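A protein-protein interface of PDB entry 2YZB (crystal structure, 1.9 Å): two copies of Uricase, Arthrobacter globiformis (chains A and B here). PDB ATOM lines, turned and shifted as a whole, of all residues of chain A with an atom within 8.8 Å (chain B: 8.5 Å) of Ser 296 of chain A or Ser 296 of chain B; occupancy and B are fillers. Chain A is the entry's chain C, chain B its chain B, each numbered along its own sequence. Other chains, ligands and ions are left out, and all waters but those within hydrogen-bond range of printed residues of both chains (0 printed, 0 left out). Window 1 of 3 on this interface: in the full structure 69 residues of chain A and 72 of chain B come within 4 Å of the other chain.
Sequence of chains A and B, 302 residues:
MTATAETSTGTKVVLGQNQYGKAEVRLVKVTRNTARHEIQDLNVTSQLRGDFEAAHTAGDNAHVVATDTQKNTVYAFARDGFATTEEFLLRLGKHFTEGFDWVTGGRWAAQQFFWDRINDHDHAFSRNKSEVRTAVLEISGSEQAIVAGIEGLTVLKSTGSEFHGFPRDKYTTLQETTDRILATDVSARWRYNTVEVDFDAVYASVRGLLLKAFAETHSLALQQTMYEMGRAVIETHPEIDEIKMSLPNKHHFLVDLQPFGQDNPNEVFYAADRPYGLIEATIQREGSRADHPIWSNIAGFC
The side-chain amide oxygen of Gln 17 of chain B sits at hydrogen-bond distance from the side-chain amide nitrogen of Asn 297 of chain B (3.2 Å).
The side-chain amino group (NZ) of Lys 244 of chain B lies within hydrogen-bond range of the side-chain amide oxygen (OE1) of Gln 17 of chain A (3.4 Å).
The side-chain hydroxyl (OG) of Ser 296 of chain A sits at hydrogen-bond distance from the side-chain hydroxyl (OG) of Ser 296 of chain B, at 2.8 Å.
Of the printed residues of chain B, Gln 17 of chain A touches Lys 244.
Of the printed residues of chain B, Lys 244 of chain A touches Gln 17.
Of chain B, only Ser 296 (2.8 Å) comes within 4 Å of Ser 296 of chain A.
Printed residues of chain A within 4 Å of Gln 17 of chain B: Lys 244.
Of the printed residues of chain A, Lys 244 of chain B touches Gln 17 (3.4 Å).
Of the printed residues of chain A, Ser 296 of chain B touches Ser 296.
The nearest printed residue of chain A that does not touch Lys 244 of chain B is Ser 296 of chain A (7.5 Å).
Among the printed residues, merely in contact across the chains: Lys 244 of chain A with Gln 17 of chain B (3.9 Å).
Gln 17 of chain A touches Lys 244 of chain B, and with the chains exchanged Lys 244 of chain A touches Gln 17 of chain B.
Ser 296 of chain A touches its own counterpart, Ser 296 of chain B.
Positions printed for both chains: 17, 19, 49, 107, 138, 244, 291, 292, 293, 294, 295, 296 and 297.
Of the 3 pairs that touch across the chains among the printed residues, 3 have their exchanged pair printed and touching as well.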
ATOM      1  N   GLN A  17       9.925  19.511  -5.563  1.00  0.00           N
ATOM      2  CA  GLN A  17       8.733  19.675  -4.745  1.00  0.00           C
ATOM      3  C   GLN A  17       9.008  20.818  -3.773  1.00  0.00           C
ATOM      4  O   GLN A  17      10.152  21.021  -3.352  1.00  0.00           O
ATOM      5  CB  GLN A  17       8.449  18.398  -3.954  1.00  0.00           C
ATOM      6  CG  GLN A  17       8.259  17.158  -4.807  1.00  0.00           C
ATOM      7  CD  GLN A  17       8.180  15.894  -3.971  1.00  0.00           C
ATOM      8  OE1 GLN A  17       9.105  15.572  -3.220  1.00  0.00           O
ATOM      9  NE2 GLN A  17       7.072  15.169  -4.095  1.00  0.00           N
ATOM     10  N   GLN A  19       6.772  23.713  -0.782  1.00  0.00           N
ATOM     11  CA  GLN A  19       5.562  24.210  -0.137  1.00  0.00           C
ATOM     12  C   GLN A  19       5.980  25.234   0.898  1.00  0.00           C
ATOM     13  O   GLN A  19       7.105  25.193   1.386  1.00  0.00           O
ATOM     14  CB  GLN A  19       4.802  23.071   0.546  1.00  0.00           C
ATOM     15  CG  GLN A  19       5.608  22.293   1.573  1.00  0.00           C
ATOM     16  CD  GLN A  19       4.822  21.127   2.147  1.00  0.00           C
ATOM     17  OE1 GLN A  19       3.969  20.560   1.473  1.00  0.00           O
ATOM     18  NE2 GLN A  19       5.119  20.753   3.388  1.00  0.00           N
ATOM     19  N   ARG A  49       0.893  24.897  -2.240  1.00  0.00           N
ATOM     20  CA  ARG A  49       1.657  24.242  -3.297  1.00  0.00           C
ATOM     21  C   ARG A  49       1.128  24.748  -4.630  1.00  0.00           C
ATOM     22  O   ARG A  49      -0.065  25.027  -4.767  1.00  0.00           O
ATOM     23  CB  ARG A  49       1.491  22.719  -3.226  1.00  0.00           C
ATOM     24  CG  ARG A  49       2.041  22.088  -1.964  1.00  0.00           C
ATOM     25  CD  ARG A  49       1.682  20.612  -1.872  1.00  0.00           C
ATOM     26  NE  ARG A  49       2.116  20.030  -0.601  1.00  0.00           N
ATOM     27  CZ  ARG A  49       1.763  18.824  -0.171  1.00  0.00           C
ATOM     28  NH1 ARG A  49       0.967  18.064  -0.909  1.00  0.00           N
ATOM     29  NH2 ARG A  49       2.209  18.374   0.994  1.00  0.00           N
ATOM     30  N   ARG A 107      -1.301  21.695   2.011  1.00  0.00           N
ATOM     31  CA  ARG A 107      -1.447  20.820   3.164  1.00  0.00           C
ATOM     32  C   ARG A 107      -1.804  21.692   4.353  1.00  0.00           C
ATOM     33  O   ARG A 107      -1.081  22.632   4.685  1.00  0.00           O
ATOM     34  CB  ARG A 107      -0.131  20.087   3.428  1.00  0.00           C
ATOM     35  CG  ARG A 107      -0.163  19.096   4.580  1.00  0.00           C
ATOM     36  CD  ARG A 107       1.247  18.633   4.902  1.00  0.00           C
ATOM     37  NE  ARG A 107       1.303  17.701   6.031  1.00  0.00           N
ATOM     38  CZ  ARG A 107       1.186  16.379   5.931  1.00  0.00           C
ATOM     39  NH1 ARG A 107       1.002  15.805   4.744  1.00  0.00           N
ATOM     40  NH2 ARG A 107       1.265  15.624   7.023  1.00  0.00           N
ATOM     41  N   GLU A 138      -4.908  17.390   2.662  1.00  0.00           N
ATOM     42  CA  GLU A 138      -3.988  17.635   1.568  1.00  0.00           C
ATOM     43  C   GLU A 138      -4.808  17.718   0.284  1.00  0.00           C
ATOM     44  O   GLU A 138      -5.704  16.898   0.051  1.00  0.00           O
ATOM     45  CB  GLU A 138      -2.944  16.516   1.467  1.00  0.00           C
ATOM     46  CG  GLU A 138      -1.845  16.798   0.451  1.00  0.00           C
ATOM     47  CD  GLU A 138      -0.555  16.031   0.731  1.00  0.00           C
ATOM     48  OE1 GLU A 138      -0.010  16.158   1.852  1.00  0.00           O
ATOM     49  OE2 GLU A 138      -0.077  15.311  -0.171  1.00  0.00           O
ATOM     50  N   VAL A 147      -6.565  12.921   6.842  1.00  0.00           N
ATOM     51  CA  VAL A 147      -6.023  11.939   7.760  1.00  0.00           C
ATOM     52  C   VAL A 147      -6.221  12.484   9.171  1.00  0.00           C
ATOM     53  O   VAL A 147      -5.754  13.573   9.487  1.00  0.00           O
ATOM     54  CB  VAL A 147      -4.513  11.701   7.511  1.00  0.00           C
ATOM     55  CG1 VAL A 147      -3.883  11.025   8.720  1.00  0.00           C
ATOM     56  CG2 VAL A 147      -4.319  10.824   6.272  1.00  0.00           C
ATOM     57  N   LYS A 244      -2.318   3.889  10.392  1.00  0.00           N
ATOM     58  CA  LYS A 244      -0.910   3.664  10.665  1.00  0.00           C
ATOM     59  C   LYS A 244      -0.651   3.901  12.144  1.00  0.00           C
ATOM     60  O   LYS A 244      -1.289   4.751  12.769  1.00  0.00           O
ATOM     61  CB  LYS A 244      -0.041   4.614   9.839  1.00  0.00           C
ATOM     62  CG  LYS A 244      -0.146   4.409   8.339  1.00  0.00           C
ATOM     63  CD  LYS A 244       0.938   5.180   7.610  1.00  0.00           C
ATOM     64  CE  LYS A 244       1.025   4.757   6.148  1.00  0.00           C
ATOM     65  NZ  LYS A 244       2.246   5.326   5.505  1.00  0.00           N
ATOM     66  N   ASP A 291       0.083   3.302  -1.391  1.00  0.00           N
ATOM     67  CA  ASP A 291       0.900   4.403  -0.895  1.00  0.00           C
ATOM     68  C   ASP A 291       0.372   5.791  -1.269  1.00  0.00           C
ATOM     69  O   ASP A 291       0.905   6.454  -2.158  1.00  0.00           O
ATOM     70  CB  ASP A 291       2.334   4.231  -1.407  1.00  0.00           C
ATOM     71  CG  ASP A 291       3.298   5.233  -0.803  1.00  0.00           C
ATOM     72  OD1 ASP A 291       3.381   5.312   0.444  1.00  0.00           O
ATOM     73  OD2 ASP A 291       3.978   5.940  -1.578  1.00  0.00           O
ATOM     74  N   HIS A 292      -0.672   6.231  -0.579  1.00  0.00           N
ATOM     75  CA  HIS A 292      -1.245   7.540  -0.849  1.00  0.00           C
ATOM     76  C   HIS A 292      -0.189   8.611  -0.577  1.00  0.00           C
ATOM     77  O   HIS A 292       0.539   8.538   0.413  1.00  0.00           O
ATOM     78  CB  HIS A 292      -2.460   7.789   0.044  1.00  0.00           C
ATOM     79  CG  HIS A 292      -3.251   8.998  -0.350  1.00  0.00           C
ATOM     80  ND1 HIS A 292      -4.460   8.914  -1.008  1.00  0.00           N
ATOM     81  CD2 HIS A 292      -2.980  10.317  -0.226  1.00  0.00           C
ATOM     82  CE1 HIS A 292      -4.899  10.132  -1.273  1.00  0.00           C
ATOM     83  NE2 HIS A 292      -4.019  11.002  -0.810  1.00  0.00           N
ATOM     84  N   PRO A 293      -0.091   9.620  -1.455  1.00  0.00           N
ATOM     85  CA  PRO A 293       0.891  10.695  -1.283  1.00  0.00           C
ATOM     86  C   PRO A 293       0.790  11.519   0.008  1.00  0.00           C
ATOM     87  O   PRO A 293       1.780  12.108   0.437  1.00  0.00           O
ATOM     88  CB  PRO A 293       0.695  11.548  -2.539  1.00  0.00           C
ATOM     89  CG  PRO A 293      -0.733  11.297  -2.906  1.00  0.00           C
ATOM     90  CD  PRO A 293      -0.856   9.813  -2.697  1.00  0.00           C
ATOM     91  N   ILE A 294      -0.382  11.551   0.636  1.00  0.00           N
ATOM     92  CA  ILE A 294      -0.541  12.331   1.865  1.00  0.00           C
ATOM     93  C   ILE A 294       0.396  11.868   2.983  1.00  0.00           C
ATOM     94  O   ILE A 294       0.732  12.645   3.880  1.00  0.00           O
ATOM     95  CB  ILE A 294      -2.005  12.290   2.392  1.00  0.00           C
ATOM     96  CG1 ILE A 294      -2.214  13.387   3.445  1.00  0.00           C
ATOM     97  CG2 ILE A 294      -2.301  10.934   3.026  1.00  0.00           C
ATOM     98  CD1 ILE A 294      -3.676  13.646   3.787  1.00  0.00           C
ATOM     99  N   TRP A 295       0.827  10.610   2.923  1.00  0.00           N
ATOM    100  CA  TRP A 295       1.715  10.063   3.945  1.00  0.00           C
ATOM    101  C   TRP A 295       3.153  10.553   3.845  1.00  0.00           C
ATOM    102  O   TRP A 295       3.895  10.497   4.824  1.00  0.00           O
ATOM    103  CB  TRP A 295       1.709   8.532   3.901  1.00  0.00           C
ATOM    104  CG  TRP A 295       0.384   7.931   4.231  1.00  0.00           C
ATOM    105  CD1 TRP A 295      -0.413   7.197   3.400  1.00  0.00           C
ATOM    106  CD2 TRP A 295      -0.307   8.019   5.479  1.00  0.00           C
ATOM    107  NE1 TRP A 295      -1.560   6.821   4.055  1.00  0.00           N
ATOM    108  CE2 TRP A 295      -1.520   7.312   5.334  1.00  0.00           C
ATOM    109  CE3 TRP A 295      -0.019   8.627   6.710  1.00  0.00           C
ATOM    110  CZ2 TRP A 295      -2.449   7.194   6.375  1.00  0.00           C
ATOM    111  CZ3 TRP A 295      -0.940   8.511   7.745  1.00  0.00           C
ATOM    112  CH2 TRP A 295      -2.142   7.799   7.570  1.00  0.00           C
ATOM    113  N   SER A 296       3.550  11.039   2.677  1.00  0.00           N
ATOM    114  CA  SER A 296       4.919  11.516   2.500  1.00  0.00           C
ATOM    115  C   SER A 296       5.109  13.007   2.764  1.00  0.00           C
ATOM    116  O   SER A 296       6.228  13.458   3.022  1.00  0.00           O
ATOM    117  CB  SER A 296       5.410  11.170   1.092  1.00  0.00           C
ATOM    118  OG  SER A 296       5.468   9.763   0.919  1.00  0.00           O
ATOM    119  N   ASN A 297       4.024  13.773   2.706  1.00  0.00           N
ATOM    120  CA  ASN A 297       4.100  15.213   2.945  1.00  0.00           C
ATOM    121  C   ASN A 297       4.933  15.894   1.857  1.00  0.00           C
ATOM    122  O   ASN A 297       4.433  16.198   0.776  1.00  0.00           O
ATOM    123  CB  ASN A 297       4.730  15.488   4.319  1.00  0.00           C
ATOM    124  CG  ASN A 297       4.771  16.969   4.662  1.00  0.00           C
ATOM    125  OD1 ASN A 297       5.101  17.805   3.821  1.00  0.00           O
ATOM    126  ND2 ASN A 297       4.448  17.297   5.908  1.00  0.00           N
ATOM    127  N   GLN B  17       2.836  -1.833   5.008  1.00  0.00           N
ATOM    128  CA  GLN B  17       4.213  -1.513   5.350  1.00  0.00           C
ATOM    129  C   GLN B  17       4.367  -1.604   6.865  1.00  0.00           C
ATOM    130  O   GLN B  17       3.463  -1.232   7.609  1.00  0.00           O
ATOM    131  CB  GLN B  17       4.564  -0.098   4.867  1.00  0.00           C
ATOM    132  CG  GLN B  17       4.321   0.125   3.373  1.00  0.00           C
ATOM    133  CD  GLN B  17       4.580   1.560   2.923  1.00  0.00           C
ATOM    134  OE1 GLN B  17       3.972   2.508   3.434  1.00  0.00           O
ATOM    135  NE2 GLN B  17       5.478   1.724   1.954  1.00  0.00           N
ATOM    136  N   GLN B  19       7.697  -1.955  10.157  1.00  0.00           N
ATOM    137  CA  GLN B  19       9.105  -1.985  10.516  1.00  0.00           C
ATOM    138  C   GLN B  19       9.179  -1.878  12.033  1.00  0.00           C
ATOM    139  O   GLN B  19       8.259  -1.353  12.671  1.00  0.00           O
ATOM    140  CB  GLN B  19       9.857  -0.821   9.843  1.00  0.00           C
ATOM    141  CG  GLN B  19       9.227   0.558  10.046  1.00  0.00           C
ATOM    142  CD  GLN B  19       9.955   1.665   9.293  1.00  0.00           C
ATOM    143  OE1 GLN B  19      10.295   1.516   8.117  1.00  0.00           O
ATOM    144  NE2 GLN B  19      10.180   2.791   9.962  1.00  0.00           N
ATOM    145  N   ARG B  49      12.988  -4.525   8.227  1.00  0.00           N
ATOM    146  CA  ARG B  49      11.860  -4.712   7.331  1.00  0.00           C
ATOM    147  C   ARG B  49      12.002  -6.100   6.717  1.00  0.00           C
ATOM    148  O   ARG B  49      13.112  -6.580   6.497  1.00  0.00           O
ATOM    149  CB  ARG B  49      11.864  -3.647   6.229  1.00  0.00           C
ATOM    150  CG  ARG B  49      11.561  -2.243   6.720  1.00  0.00           C
ATOM    151  CD  ARG B  49      11.904  -1.189   5.682  1.00  0.00           C
ATOM    152  NE  ARG B  49      11.651   0.159   6.191  1.00  0.00           N
ATOM    153  CZ  ARG B  49      12.052   1.275   5.591  1.00  0.00           C
ATOM    154  NH1 ARG B  49      12.733   1.214   4.454  1.00  0.00           N
ATOM    155  NH2 ARG B  49      11.765   2.455   6.124  1.00  0.00           N
ATOM    156  N   ARG B 107      15.849   0.441   8.069  1.00  0.00           N
ATOM    157  CA  ARG B 107      16.199   1.842   8.160  1.00  0.00           C
ATOM    158  C   ARG B 107      17.016   2.002   9.426  1.00  0.00           C
ATOM    159  O   ARG B 107      16.553   1.663  10.508  1.00  0.00           O
ATOM    160  CB  ARG B 107      14.936   2.702   8.242  1.00  0.00           C
ATOM    161  CG  ARG B 107      15.197   4.199   8.391  1.00  0.00           C
ATOM    162  CD  ARG B 107      13.891   4.992   8.347  1.00  0.00           C
ATOM    163  NE  ARG B 107      14.103   6.430   8.497  1.00  0.00           N
ATOM    164  CZ  ARG B 107      14.399   7.037   9.646  1.00  0.00           C
ATOM    165  NH1 ARG B 107      14.520   6.336  10.769  1.00  0.00           N
ATOM    166  NH2 ARG B 107      14.582   8.353   9.672  1.00  0.00           N
ATOM    167  N   VAL B 136      21.065   8.754   7.616  1.00  0.00           N
ATOM    168  CA  VAL B 136      20.048   7.732   7.515  1.00  0.00           C
ATOM    169  C   VAL B 136      20.424   6.801   6.381  1.00  0.00           C
ATOM    170  O   VAL B 136      20.756   7.249   5.278  1.00  0.00           O
ATOM    171  CB  VAL B 136      18.649   8.326   7.230  1.00  0.00           C
ATOM    172  CG1 VAL B 136      17.623   7.204   7.157  1.00  0.00           C
ATOM    173  CG2 VAL B 136      18.260   9.314   8.329  1.00  0.00           C
ATOM    174  N   GLU B 138      19.084   3.401   4.243  1.00  0.00           N
ATOM    175  CA  GLU B 138      17.935   2.566   3.960  1.00  0.00           C
ATOM    176  C   GLU B 138      18.357   1.479   2.983  1.00  0.00           C
ATOM    177  O   GLU B 138      18.992   1.756   1.962  1.00  0.00           O
ATOM    178  CB  GLU B 138      16.784   3.380   3.370  1.00  0.00           C
ATOM    179  CG  GLU B 138      15.566   2.524   3.060  1.00  0.00           C
ATOM    180  CD  GLU B 138      14.325   3.340   2.748  1.00  0.00           C
ATOM    181  OE1 GLU B 138      13.870   4.096   3.636  1.00  0.00           O
ATOM    182  OE2 GLU B 138      13.803   3.217   1.617  1.00  0.00           O
ATOM    183  N   LYS B 244      17.013  18.511   0.418  1.00  0.00           N
ATOM    184  CA  LYS B 244      15.738  19.013   0.895  1.00  0.00           C
ATOM    185  C   LYS B 244      15.969  19.910   2.098  1.00  0.00           C
ATOM    186  O   LYS B 244      16.757  19.582   2.987  1.00  0.00           O
ATOM    187  CB  LYS B 244      14.819  17.856   1.291  1.00  0.00           C
ATOM    188  CG  LYS B 244      14.336  17.003   0.120  1.00  0.00           C
ATOM    189  CD  LYS B 244      13.440  15.879   0.615  1.00  0.00           C
ATOM    190  CE  LYS B 244      12.745  15.154  -0.529  1.00  0.00           C
ATOM    191  NZ  LYS B 244      11.811  16.053  -1.264  1.00  0.00           N
ATOM    192  N   ASP B 291      11.121  11.096  -6.381  1.00  0.00           N
ATOM    193  CA  ASP B 291      10.543  10.510  -5.176  1.00  0.00           C
ATOM    194  C   ASP B 291      11.224   9.236  -4.692  1.00  0.00           C
ATOM    195  O   ASP B 291      10.647   8.152  -4.770  1.00  0.00           O
ATOM    196  CB  ASP B 291       9.053  10.233  -5.390  1.00  0.00           C
ATOM    197  CG  ASP B 291       8.345   9.821  -4.109  1.00  0.00           C
ATOM    198  OD1 ASP B 291       8.257  10.654  -3.180  1.00  0.00           O
ATOM    199  OD2 ASP B 291       7.879   8.665  -4.028  1.00  0.00           O
ATOM    200  N   HIS B 292      12.446   9.363  -4.188  1.00  0.00           N
ATOM    201  CA  HIS B 292      13.162   8.199  -3.681  1.00  0.00           C
ATOM    202  C   HIS B 292      12.440   7.723  -2.422  1.00  0.00           C
ATOM    203  O   HIS B 292      12.005   8.532  -1.600  1.00  0.00           O
ATOM    204  CB  HIS B 292      14.610   8.554  -3.339  1.00  0.00           C
ATOM    205  CG  HIS B 292      15.471   7.361  -3.063  1.00  0.00           C
ATOM    206  ND1 HIS B 292      16.093   6.644  -4.061  1.00  0.00           N
ATOM    207  CD2 HIS B 292      15.784   6.737  -1.902  1.00  0.00           C
ATOM    208  CE1 HIS B 292      16.754   5.632  -3.529  1.00  0.00           C
ATOM    209  NE2 HIS B 292      16.582   5.666  -2.220  1.00  0.00           N
ATOM    210  N   PRO B 293      12.303   6.397  -2.258  1.00  0.00           N
ATOM    211  CA  PRO B 293      11.631   5.778  -1.109  1.00  0.00           C
ATOM    212  C   PRO B 293      12.166   6.185   0.261  1.00  0.00           C
ATOM    213  O   PRO B 293      11.437   6.142   1.253  1.00  0.00           O
ATOM    214  CB  PRO B 293      11.816   4.284  -1.368  1.00  0.00           C
ATOM    215  CG  PRO B 293      11.864   4.204  -2.855  1.00  0.00           C
ATOM    216  CD  PRO B 293      12.751   5.368  -3.211  1.00  0.00           C
ATOM    217  N   ILE B 294      13.432   6.586   0.316  1.00  0.00           N
ATOM    218  CA  ILE B 294      14.048   6.965   1.584  1.00  0.00           C
ATOM    219  C   ILE B 294      13.411   8.197   2.224  1.00  0.00           C
ATOM    220  O   ILE B 294      13.581   8.440   3.417  1.00  0.00           O
ATOM    221  CB  ILE B 294      15.569   7.207   1.414  1.00  0.00           C
ATOM    222  CG1 ILE B 294      16.262   7.119   2.778  1.00  0.00           C
ATOM    223  CG2 ILE B 294      15.815   8.575   0.788  1.00  0.00           C
ATOM    224  CD1 ILE B 294      17.782   7.094   2.703  1.00  0.00           C
ATOM    225  N   TRP B 295      12.674   8.975   1.439  1.00  0.00           N
ATOM    226  CA  TRP B 295      12.029  10.163   1.981  1.00  0.00           C
ATOM    227  C   TRP B 295      10.677   9.837   2.626  1.00  0.00           C
ATOM    228  O   TRP B 295       9.954  10.733   3.059  1.00  0.00           O
ATOM    229  CB  TRP B 295      11.850  11.219   0.885  1.00  0.00           C
ATOM    230  CG  TRP B 295      13.150  11.705   0.290  1.00  0.00           C
ATOM    231  CD1 TRP B 295      13.570  11.547  -0.998  1.00  0.00           C
ATOM    232  CD2 TRP B 295      14.175  12.460   0.955  1.00  0.00           C
ATOM    233  NE1 TRP B 295      14.788  12.158  -1.181  1.00  0.00           N
ATOM    234  CE2 TRP B 295      15.183  12.726   0.001  1.00  0.00           C
ATOM    235  CE3 TRP B 295      14.338  12.939   2.264  1.00  0.00           C
ATOM    236  CZ2 TRP B 295      16.340  13.453   0.311  1.00  0.00           C
ATOM    237  CZ3 TRP B 295      15.490  13.662   2.572  1.00  0.00           C
ATOM    238  CH2 TRP B 295      16.475  13.911   1.597  1.00  0.00           C
ATOM    239  N   SER B 296      10.347   8.551   2.698  1.00  0.00           N
ATOM    240  CA  SER B 296       9.088   8.116   3.301  1.00  0.00           C
ATOM    241  C   SER B 296       9.330   7.162   4.474  1.00  0.00           C
ATOM    242  O   SER B 296      10.457   6.712   4.695  1.00  0.00           O
ATOM    243  CB  SER B 296       8.208   7.429   2.254  1.00  0.00           C
ATOM    244  OG  SER B 296       7.819   8.339   1.238  1.00  0.00           O
ATOM    245  N   ASN B 297       8.266   6.860   5.215  1.00  0.00           N
ATOM    246  CA  ASN B 297       8.332   5.962   6.368  1.00  0.00           C
ATOM    247  C   ASN B 297       9.588   6.186   7.216  1.00  0.00           C
ATOM    248  O   ASN B 297      10.294   5.188   7.498  1.00  0.00           O
ATOM    249  CB  ASN B 297       8.288   4.499   5.910  1.00  0.00           C
ATOM    250  CG  ASN B 297       7.092   4.197   5.025  1.00  0.00           C
ATOM    251  OD1 ASN B 297       7.029   4.637   3.877  1.00  0.00           O
ATOM    252  ND2 ASN B 297       6.134   3.447   5.559  1.00  0.00           N
